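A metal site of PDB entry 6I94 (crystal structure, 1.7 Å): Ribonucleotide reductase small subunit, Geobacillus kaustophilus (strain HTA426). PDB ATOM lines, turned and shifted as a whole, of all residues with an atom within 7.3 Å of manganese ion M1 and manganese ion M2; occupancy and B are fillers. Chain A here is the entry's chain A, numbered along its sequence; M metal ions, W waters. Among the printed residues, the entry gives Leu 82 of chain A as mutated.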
ATOM      1  N   PHE A  79       1.442   1.123  25.542  1.00  0.00           N
ATOM      2  CA  PHE A  79       2.055   1.640  24.334  1.00  0.00           C
ATOM      3  C   PHE A  79       2.314   3.145  24.417  1.00  0.00           C
ATOM      4  O   PHE A  79       3.311   3.624  23.872  1.00  0.00           O
ATOM      5  CB  PHE A  79       1.202   1.318  23.102  1.00  0.00           C
ATOM      6  CG  PHE A  79       1.778   0.212  22.274  1.00  0.00           C
ATOM      7  CD1 PHE A  79       2.990   0.393  21.599  1.00  0.00           C
ATOM      8  CD2 PHE A  79       1.140  -1.003  22.182  1.00  0.00           C
ATOM      9  CE1 PHE A  79       3.534  -0.629  20.842  1.00  0.00           C
ATOM     10  CE2 PHE A  79       1.678  -2.036  21.417  1.00  0.00           C
ATOM     11  CZ  PHE A  79       2.874  -1.854  20.754  1.00  0.00           C
ATOM     12  N   LEU A  82       5.482   3.482  26.271  1.00  0.00           N
ATOM     13  CA  LEU A  82       6.600   2.967  25.489  1.00  0.00           C
ATOM     14  C   LEU A  82       7.052   3.994  24.473  1.00  0.00           C
ATOM     15  O   LEU A  82       8.240   4.306  24.368  1.00  0.00           O
ATOM     16  CB  LEU A  82       6.232   1.651  24.807  1.00  0.00           C
ATOM     17  CG  LEU A  82       7.358   0.898  24.067  1.00  0.00           C
ATOM     18  CD1 LEU A  82       6.987  -0.575  24.015  1.00  0.00           C
ATOM     19  CD2 LEU A  82       7.553   1.407  22.695  1.00  0.00           C
ATOM     20  N   GLU A  83       6.097   4.560  23.730  1.00  0.00           N
ATOM     21  CA  GLU A  83       6.476   5.463  22.638  1.00  0.00           C
ATOM     22  C   GLU A  83       7.055   6.752  23.204  1.00  0.00           C
ATOM     23  O   GLU A  83       8.016   7.302  22.658  1.00  0.00           O
ATOM     24  CB  GLU A  83       5.283   5.740  21.737  1.00  0.00           C
ATOM     25  CG  GLU A  83       4.638   4.449  21.132  1.00  0.00           C
ATOM     26  CD  GLU A  83       5.536   3.637  20.203  1.00  0.00           C
ATOM     27  OE1 GLU A  83       5.192   2.454  19.968  1.00  0.00           O
ATOM     28  OE2 GLU A  83       6.580   4.158  19.685  1.00  0.00           O
ATOM     29  N   VAL A  86      10.688   5.942  24.402  1.00  0.00           N
ATOM     30  CA  VAL A  86      11.687   5.744  23.356  1.00  0.00           C
ATOM     31  C   VAL A  86      11.921   7.046  22.586  1.00  0.00           C
ATOM     32  O   VAL A  86      13.008   7.253  22.027  1.00  0.00           O
ATOM     33  CB  VAL A  86      11.317   4.585  22.407  1.00  0.00           C
ATOM     34  CG1 VAL A  86      11.331   3.251  23.145  1.00  0.00           C
ATOM     35  CG2 VAL A  86       9.985   4.820  21.659  1.00  0.00           C
ATOM     36  N   THR A  87      10.921   7.948  22.542  1.00  0.00           N
ATOM     37  CA  THR A  87      11.168   9.246  21.925  1.00  0.00           C
ATOM     38  C   THR A  87      12.241   9.994  22.689  1.00  0.00           C
ATOM     39  O   THR A  87      13.189  10.551  22.089  1.00  0.00           O
ATOM     40  CB  THR A  87       9.868  10.089  21.880  1.00  0.00           C
ATOM     41  OG1 THR A  87       8.894   9.450  21.076  1.00  0.00           O
ATOM     42  CG2 THR A  87      10.125  11.457  21.239  1.00  0.00           C
ATOM     43  N   PHE A 112      14.646   8.076  12.901  1.00  0.00           N
ATOM     44  CA  PHE A 112      14.233   7.224  14.028  1.00  0.00           C
ATOM     45  C   PHE A 112      13.496   8.052  15.075  1.00  0.00           C
ATOM     46  O   PHE A 112      12.372   7.698  15.507  1.00  0.00           O
ATOM     47  CB  PHE A 112      15.498   6.558  14.574  1.00  0.00           C
ATOM     48  CG  PHE A 112      15.298   5.417  15.534  1.00  0.00           C
ATOM     49  CD1 PHE A 112      15.957   4.223  15.333  1.00  0.00           C
ATOM     50  CD2 PHE A 112      14.569   5.559  16.682  1.00  0.00           C
ATOM     51  CE1 PHE A 112      15.822   3.169  16.242  1.00  0.00           C
ATOM     52  CE2 PHE A 112      14.443   4.515  17.584  1.00  0.00           C
ATOM     53  CZ  PHE A 112      15.068   3.330  17.371  1.00  0.00           C
ATOM     54  N   ASP A 115      10.182   9.395  13.740  1.00  0.00           N
ATOM     55  CA  ASP A 115       9.203   8.308  13.768  1.00  0.00           C
ATOM     56  C   ASP A 115       8.581   8.162  15.163  1.00  0.00           C
ATOM     57  O   ASP A 115       7.355   8.084  15.321  1.00  0.00           O
ATOM     58  CB  ASP A 115       9.868   6.972  13.346  1.00  0.00           C
ATOM     59  CG  ASP A 115      10.234   6.896  11.902  1.00  0.00           C
ATOM     60  OD1 ASP A 115       9.827   7.716  11.080  1.00  0.00           O
ATOM     61  OD2 ASP A 115      10.969   5.935  11.572  1.00  0.00           O
ATOM     62  N   GLU A 116       9.421   8.114  16.212  1.00  0.00           N
ATOM     63  CA  GLU A 116       8.893   7.905  17.553  1.00  0.00           C
ATOM     64  C   GLU A 116       7.979   9.051  17.968  1.00  0.00           C
ATOM     65  O   GLU A 116       6.969   8.828  18.633  1.00  0.00           O
ATOM     66  CB  GLU A 116       9.999   7.795  18.596  1.00  0.00           C
ATOM     67  CG  GLU A 116      10.983   6.689  18.376  1.00  0.00           C
ATOM     68  CD  GLU A 116      10.413   5.274  18.269  1.00  0.00           C
ATOM     69  OE1 GLU A 116      11.227   4.400  18.076  1.00  0.00           O
ATOM     70  OE2 GLU A 116       9.198   5.024  18.403  1.00  0.00           O
ATOM     71  N   ALA A 117       8.313  10.291  17.575  1.00  0.00           N
ATOM     72  CA  ALA A 117       7.401  11.409  17.841  1.00  0.00           C
ATOM     73  C   ALA A 117       6.019  11.163  17.254  1.00  0.00           C
ATOM     74  O   ALA A 117       4.974  11.439  17.895  1.00  0.00           O
ATOM     75  CB  ALA A 117       7.982  12.700  17.275  1.00  0.00           C
ATOM     76  N   LYS A 118       5.977  10.687  16.004  1.00  0.00           N
ATOM     77  CA  LYS A 118       4.696  10.378  15.371  1.00  0.00           C
ATOM     78  C   LYS A 118       3.986   9.257  16.108  1.00  0.00           C
ATOM     79  O   LYS A 118       2.750   9.213  16.149  1.00  0.00           O
ATOM     80  CB  LYS A 118       4.939  10.000  13.895  1.00  0.00           C
ATOM     81  CG  LYS A 118       5.423  11.198  13.083  1.00  0.00           C
ATOM     82  CD  LYS A 118       5.334  10.968  11.534  1.00  0.00           C
ATOM     83  CE  LYS A 118       6.171   9.809  11.065  1.00  0.00           C
ATOM     84  NZ  LYS A 118       6.167   9.811   9.553  1.00  0.00           N
ATOM     85  N   HIS A 119       4.742   8.280  16.620  1.00  0.00           N
ATOM     86  CA  HIS A 119       4.107   7.168  17.340  1.00  0.00           C
ATOM     87  C   HIS A 119       3.462   7.637  18.634  1.00  0.00           C
ATOM     88  O   HIS A 119       2.335   7.227  18.948  1.00  0.00           O
ATOM     89  CB  HIS A 119       5.129   6.110  17.661  1.00  0.00           C
ATOM     90  CG  HIS A 119       5.747   5.494  16.456  1.00  0.00           C
ATOM     91  ND1 HIS A 119       6.756   4.554  16.532  1.00  0.00           N
ATOM     92  CD2 HIS A 119       5.549   5.727  15.138  1.00  0.00           C
ATOM     93  CE1 HIS A 119       7.139   4.229  15.311  1.00  0.00           C
ATOM     94  NE2 HIS A 119       6.424   4.927  14.448  1.00  0.00           N
ATOM     95  N   VAL A 120       4.164   8.466  19.394  1.00  0.00           N
ATOM     96  CA  VAL A 120       3.576   9.120  20.587  1.00  0.00           C
ATOM     97  C   VAL A 120       2.330   9.885  20.197  1.00  0.00           C
ATOM     98  O   VAL A 120       1.284   9.845  20.905  1.00  0.00           O
ATOM     99  CB  VAL A 120       4.603  10.082  21.226  1.00  0.00           C
ATOM    100  CG1 VAL A 120       3.928  10.905  22.375  1.00  0.00           C
ATOM    101  CG2 VAL A 120       5.776   9.363  21.717  1.00  0.00           C
ATOM    102  N   PHE A 123      -0.904   7.598  19.345  1.00  0.00           N
ATOM    103  CA  PHE A 123      -1.668   7.048  20.467  1.00  0.00           C
ATOM    104  C   PHE A 123      -2.360   8.152  21.255  1.00  0.00           C
ATOM    105  O   PHE A 123      -3.461   7.952  21.762  1.00  0.00           O
ATOM    106  CB  PHE A 123      -0.783   6.231  21.384  1.00  0.00           C
ATOM    107  CG  PHE A 123      -0.442   4.850  20.843  1.00  0.00           C
ATOM    108  CD1 PHE A 123      -1.415   3.894  20.686  1.00  0.00           C
ATOM    109  CD2 PHE A 123       0.871   4.528  20.504  1.00  0.00           C
ATOM    110  CE1 PHE A 123      -1.100   2.625  20.170  1.00  0.00           C
ATOM    111  CE2 PHE A 123       1.184   3.280  20.001  1.00  0.00           C
ATOM    112  CZ  PHE A 123       0.175   2.323  19.846  1.00  0.00           C
ATOM    113  N   TYR A 176      16.998  -1.165  24.445  1.00  0.00           N
ATOM    114  CA  TYR A 176      16.106  -0.332  23.655  1.00  0.00           C
ATOM    115  C   TYR A 176      15.574  -1.094  22.445  1.00  0.00           C
ATOM    116  O   TYR A 176      14.355  -1.249  22.279  1.00  0.00           O
ATOM    117  CB  TYR A 176      16.855   0.925  23.218  1.00  0.00           C
ATOM    118  CG  TYR A 176      16.044   2.026  22.590  1.00  0.00           C
ATOM    119  CD1 TYR A 176      16.023   3.297  23.151  1.00  0.00           C
ATOM    120  CD2 TYR A 176      15.353   1.817  21.420  1.00  0.00           C
ATOM    121  CE1 TYR A 176      15.322   4.320  22.559  1.00  0.00           C
ATOM    122  CE2 TYR A 176      14.640   2.829  20.813  1.00  0.00           C
ATOM    123  CZ  TYR A 176      14.627   4.070  21.369  1.00  0.00           C
ATOM    124  OH  TYR A 176      13.937   5.102  20.757  1.00  0.00           O
ATOM    125  N   ASN A 177      16.467  -1.572  21.591  1.00  0.00           N
ATOM    126  CA  ASN A 177      16.050  -2.060  20.269  1.00  0.00           C
ATOM    127  C   ASN A 177      15.590  -3.507  20.332  1.00  0.00           C
ATOM    128  O   ASN A 177      14.606  -3.869  19.669  1.00  0.00           O
ATOM    129  CB  ASN A 177      17.186  -1.926  19.256  1.00  0.00           C
ATOM    130  CG  ASN A 177      17.667  -0.513  19.105  1.00  0.00           C
ATOM    131  OD1 ASN A 177      18.676  -0.138  19.650  1.00  0.00           O
ATOM    132  ND2 ASN A 177      16.893   0.283  18.392  1.00  0.00           N
ATOM    133  N   GLU A 181      11.688  -2.543  21.893  1.00  0.00           N
ATOM    134  CA  GLU A 181      11.049  -2.510  20.560  1.00  0.00           C
ATOM    135  C   GLU A 181      10.918  -3.912  19.968  1.00  0.00           C
ATOM    136  O   GLU A 181       9.843  -4.274  19.485  1.00  0.00           O
ATOM    137  CB  GLU A 181      11.812  -1.580  19.619  1.00  0.00           C
ATOM    138  CG  GLU A 181      11.921  -0.157  20.213  1.00  0.00           C
ATOM    139  CD  GLU A 181      11.753   0.963  19.225  1.00  0.00           C
ATOM    140  OE1 GLU A 181      12.688   1.243  18.488  1.00  0.00           O
ATOM    141  OE2 GLU A 181      10.651   1.567  19.210  1.00  0.00           O
ATOM    142  N   ALA A 185       7.284  -4.335  22.023  1.00  0.00           N
ATOM    143  CA  ALA A 185       6.466  -3.580  21.084  1.00  0.00           C
ATOM    144  C   ALA A 185       5.995  -4.479  19.947  1.00  0.00           C
ATOM    145  O   ALA A 185       4.821  -4.474  19.580  1.00  0.00           O
ATOM    146  CB  ALA A 185       7.220  -2.380  20.521  1.00  0.00           C
ATOM    147  N   TYR A 189       2.052  -4.987  18.993  1.00  0.00           N
ATOM    148  CA  TYR A 189       1.399  -4.782  17.699  1.00  0.00           C
ATOM    149  C   TYR A 189       0.570  -5.998  17.363  1.00  0.00           C
ATOM    150  O   TYR A 189      -0.633  -5.909  17.086  1.00  0.00           O
ATOM    151  CB  TYR A 189       2.387  -4.615  16.532  1.00  0.00           C
ATOM    152  CG  TYR A 189       3.435  -3.588  16.704  1.00  0.00           C
ATOM    153  CD1 TYR A 189       3.199  -2.494  17.506  1.00  0.00           C
ATOM    154  CD2 TYR A 189       4.676  -3.724  16.086  1.00  0.00           C
ATOM    155  CE1 TYR A 189       4.145  -1.576  17.697  1.00  0.00           C
ATOM    156  CE2 TYR A 189       5.638  -2.796  16.265  1.00  0.00           C
ATOM    157  CZ  TYR A 189       5.366  -1.712  17.069  1.00  0.00           C
ATOM    158  OH  TYR A 189       6.300  -0.752  17.291  1.00  0.00           O
ATOM    159  N   LEU A 212       3.099   2.335  12.150  1.00  0.00           N
ATOM    160  CA  LEU A 212       4.097   2.226  13.199  1.00  0.00           C
ATOM    161  C   LEU A 212       4.940   0.962  13.015  1.00  0.00           C
ATOM    162  O   LEU A 212       6.163   0.986  13.160  1.00  0.00           O
ATOM    163  CB  LEU A 212       3.351   2.217  14.517  1.00  0.00           C
ATOM    164  CG  LEU A 212       3.984   2.323  15.834  1.00  0.00           C
ATOM    165  CD1 LEU A 212       2.969   2.801  16.878  1.00  0.00           C
ATOM    166  CD2 LEU A 212       4.425   0.955  16.124  1.00  0.00           C
ATOM    167  N   ASP A 215       7.496   1.504  10.294  1.00  0.00           N
ATOM    168  CA  ASP A 215       8.631   2.268  10.801  1.00  0.00           C
ATOM    169  C   ASP A 215       9.567   1.386  11.623  1.00  0.00           C
ATOM    170  O   ASP A 215      10.775   1.466  11.490  1.00  0.00           O
ATOM    171  CB  ASP A 215       8.174   3.437  11.687  1.00  0.00           C
ATOM    172  CG  ASP A 215       7.380   4.472  10.951  1.00  0.00           C
ATOM    173  OD1 ASP A 215       7.521   4.638   9.710  1.00  0.00           O
ATOM    174  OD2 ASP A 215       6.608   5.183  11.669  1.00  0.00           O
ATOM    175  N   GLU A 216       9.011   0.573  12.518  1.00  0.00           N
ATOM    176  CA  GLU A 216       9.800  -0.129  13.501  1.00  0.00           C
ATOM    177  C   GLU A 216      10.655  -1.216  12.866  1.00  0.00           C
ATOM    178  O   GLU A 216      11.696  -1.572  13.410  1.00  0.00           O
ATOM    179  CB  GLU A 216       8.893  -0.691  14.579  1.00  0.00           C
ATOM    180  CG  GLU A 216       8.284   0.446  15.429  1.00  0.00           C
ATOM    181  CD  GLU A 216       9.309   1.178  16.279  1.00  0.00           C
ATOM    182  OE1 GLU A 216      10.357   0.541  16.596  1.00  0.00           O
ATOM    183  OE2 GLU A 216       9.044   2.368  16.613  1.00  0.00           O
ATOM    184  N   GLY A 217      10.283  -1.688  11.672  1.00  0.00           N
ATOM    185  CA  GLY A 217      11.200  -2.522  10.905  1.00  0.00           C
ATOM    186  C   GLY A 217      12.557  -1.885  10.708  1.00  0.00           C
ATOM    187  O   GLY A 217      13.597  -2.497  10.944  1.00  0.00           O
ATOM    188  N   ARG A 218      12.563  -0.592  10.355  1.00  0.00           N
ATOM    189  CA  ARG A 218      13.850   0.107  10.194  1.00  0.00           C
ATOM    190  C   ARG A 218      14.584   0.223  11.512  1.00  0.00           C
ATOM    191  O   ARG A 218      15.807   0.032  11.568  1.00  0.00           O
ATOM    192  CB  ARG A 218      13.640   1.499   9.609  1.00  0.00           C
ATOM    193  CG  ARG A 218      13.134   1.498   8.205  1.00  0.00           C
ATOM    194  CD  ARG A 218      13.202   2.899   7.627  1.00  0.00           C
ATOM    195  NE  ARG A 218      12.378   3.833   8.396  1.00  0.00           N
ATOM    196  CZ  ARG A 218      11.058   3.969   8.228  1.00  0.00           C
ATOM    197  NH1 ARG A 218      10.413   3.261   7.284  1.00  0.00           N
ATOM    198  NH2 ARG A 218      10.380   4.841   8.980  1.00  0.00           N
ATOM    199  N   HIS A 219      13.867   0.591  12.579  1.00  0.00           N
ATOM    200  CA  HIS A 219      14.481   0.787  13.881  1.00  0.00           C
ATOM    201  C   HIS A 219      15.219  -0.463  14.333  1.00  0.00           C
ATOM    202  O   HIS A 219      16.310  -0.377  14.905  1.00  0.00           O
ATOM    203  CB  HIS A 219      13.412   1.144  14.908  1.00  0.00           C
ATOM    204  CG  HIS A 219      12.723   2.423  14.606  1.00  0.00           C
ATOM    205  ND1 HIS A 219      11.840   3.032  15.484  1.00  0.00           N
ATOM    206  CD2 HIS A 219      12.739   3.196  13.500  1.00  0.00           C
ATOM    207  CE1 HIS A 219      11.369   4.126  14.931  1.00  0.00           C
ATOM    208  NE2 HIS A 219      11.891   4.252  13.722  1.00  0.00           N
ATOM    209  N   ILE A 220      14.638  -1.625  14.097  1.00  0.00           N
ATOM    210  CA  ILE A 220      15.293  -2.832  14.619  1.00  0.00           C
ATOM    211  C   ILE A 220      16.544  -3.138  13.804  1.00  0.00           C
ATOM    212  O   ILE A 220      17.523  -3.654  14.340  1.00  0.00           O
ATOM    213  CB  ILE A 220      14.286  -4.009  14.647  1.00  0.00           C
ATOM    214  CG1 ILE A 220      13.160  -3.674  15.631  1.00  0.00           C
ATOM    215  CG2 ILE A 220      14.978  -5.278  15.121  1.00  0.00           C
ATOM    216  CD1 ILE A 220      11.941  -4.631  15.629  1.00  0.00           C
HETATM  217 MN    MN M   1       7.782   3.502  18.128  1.00  0.00          MN
HETATM  218 MN    MN M   2      11.161   2.373  17.405  1.00  0.00          MN
HETATM  219  O   HOH W   1       6.893   1.531  18.295  1.00  0.00           O
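Manganese ion M1 is bound by OE2 of Glu 83, OE2 of Glu 116, water W1, ND1 of His 119 and OE2 of Glu 216.
Water W1 lies within hydrogen-bond range of OE1 of Glu 83 (2.6 Å) and OH of Tyr 189 (2.6 Å).
Residues that only touch manganese ion M2: Phe 112.
The nearest printed residue that does not touch manganese ion M2 is Tyr 176 (4.9 Å).
Of the 25 residues printed, 5 come within 4 Å of manganese ion M1.
The nearest printed residue that does not touch manganese ion M1 is Val 86 (4.4 Å).
OE2 of Glu 181 binds manganese ion M2, 2.0 Å away.
The side-chain carboxylate (OE1) of Glu 116 is bound to manganese ion M2.
A ring nitrogen (ND1) of His 219 is bound to manganese ion M2, at 2.1 Å.
OE1 of Glu 216 is bound to manganese ion M2, 2.2 Å away.
Manganese ion M2 is bound by the side-chain carboxylate (OE1) of Glu 181, 2.2 Å away.
Manganese ion M2 is bound by the side-chain carboxylate (OE2) of Glu 216, at 2.3 Å.
Manganese ion M2 has six donor atoms within binding distance.
N of Glu 181 is in hydrogen-bond range of O of Tyr 176 (3.0 Å).
The backbone carbonyl oxygen (O) of Glu 83 is in hydrogen-bond range of the side-chain hydroxyl (OG1) of Thr 87.
The backbone carbonyl oxygen of Glu 116 is in hydrogen-bond range of the side-chain hydroxyl of Thr 87 (3.2 Å).
A ring nitrogen (NE2) of His 219 lies within hydrogen-bond range of the side-chain carboxylate of Asp 115.
A ring nitrogen (NE2) of His 119 sits close to the backbone carbonyl oxygen (O) of Asp 115 (3.4 Å).
A ring nitrogen (NE2) of His 119 is in hydrogen-bond range of the side-chain carboxylate (OD2) of Asp 215, at 2.8 Å.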
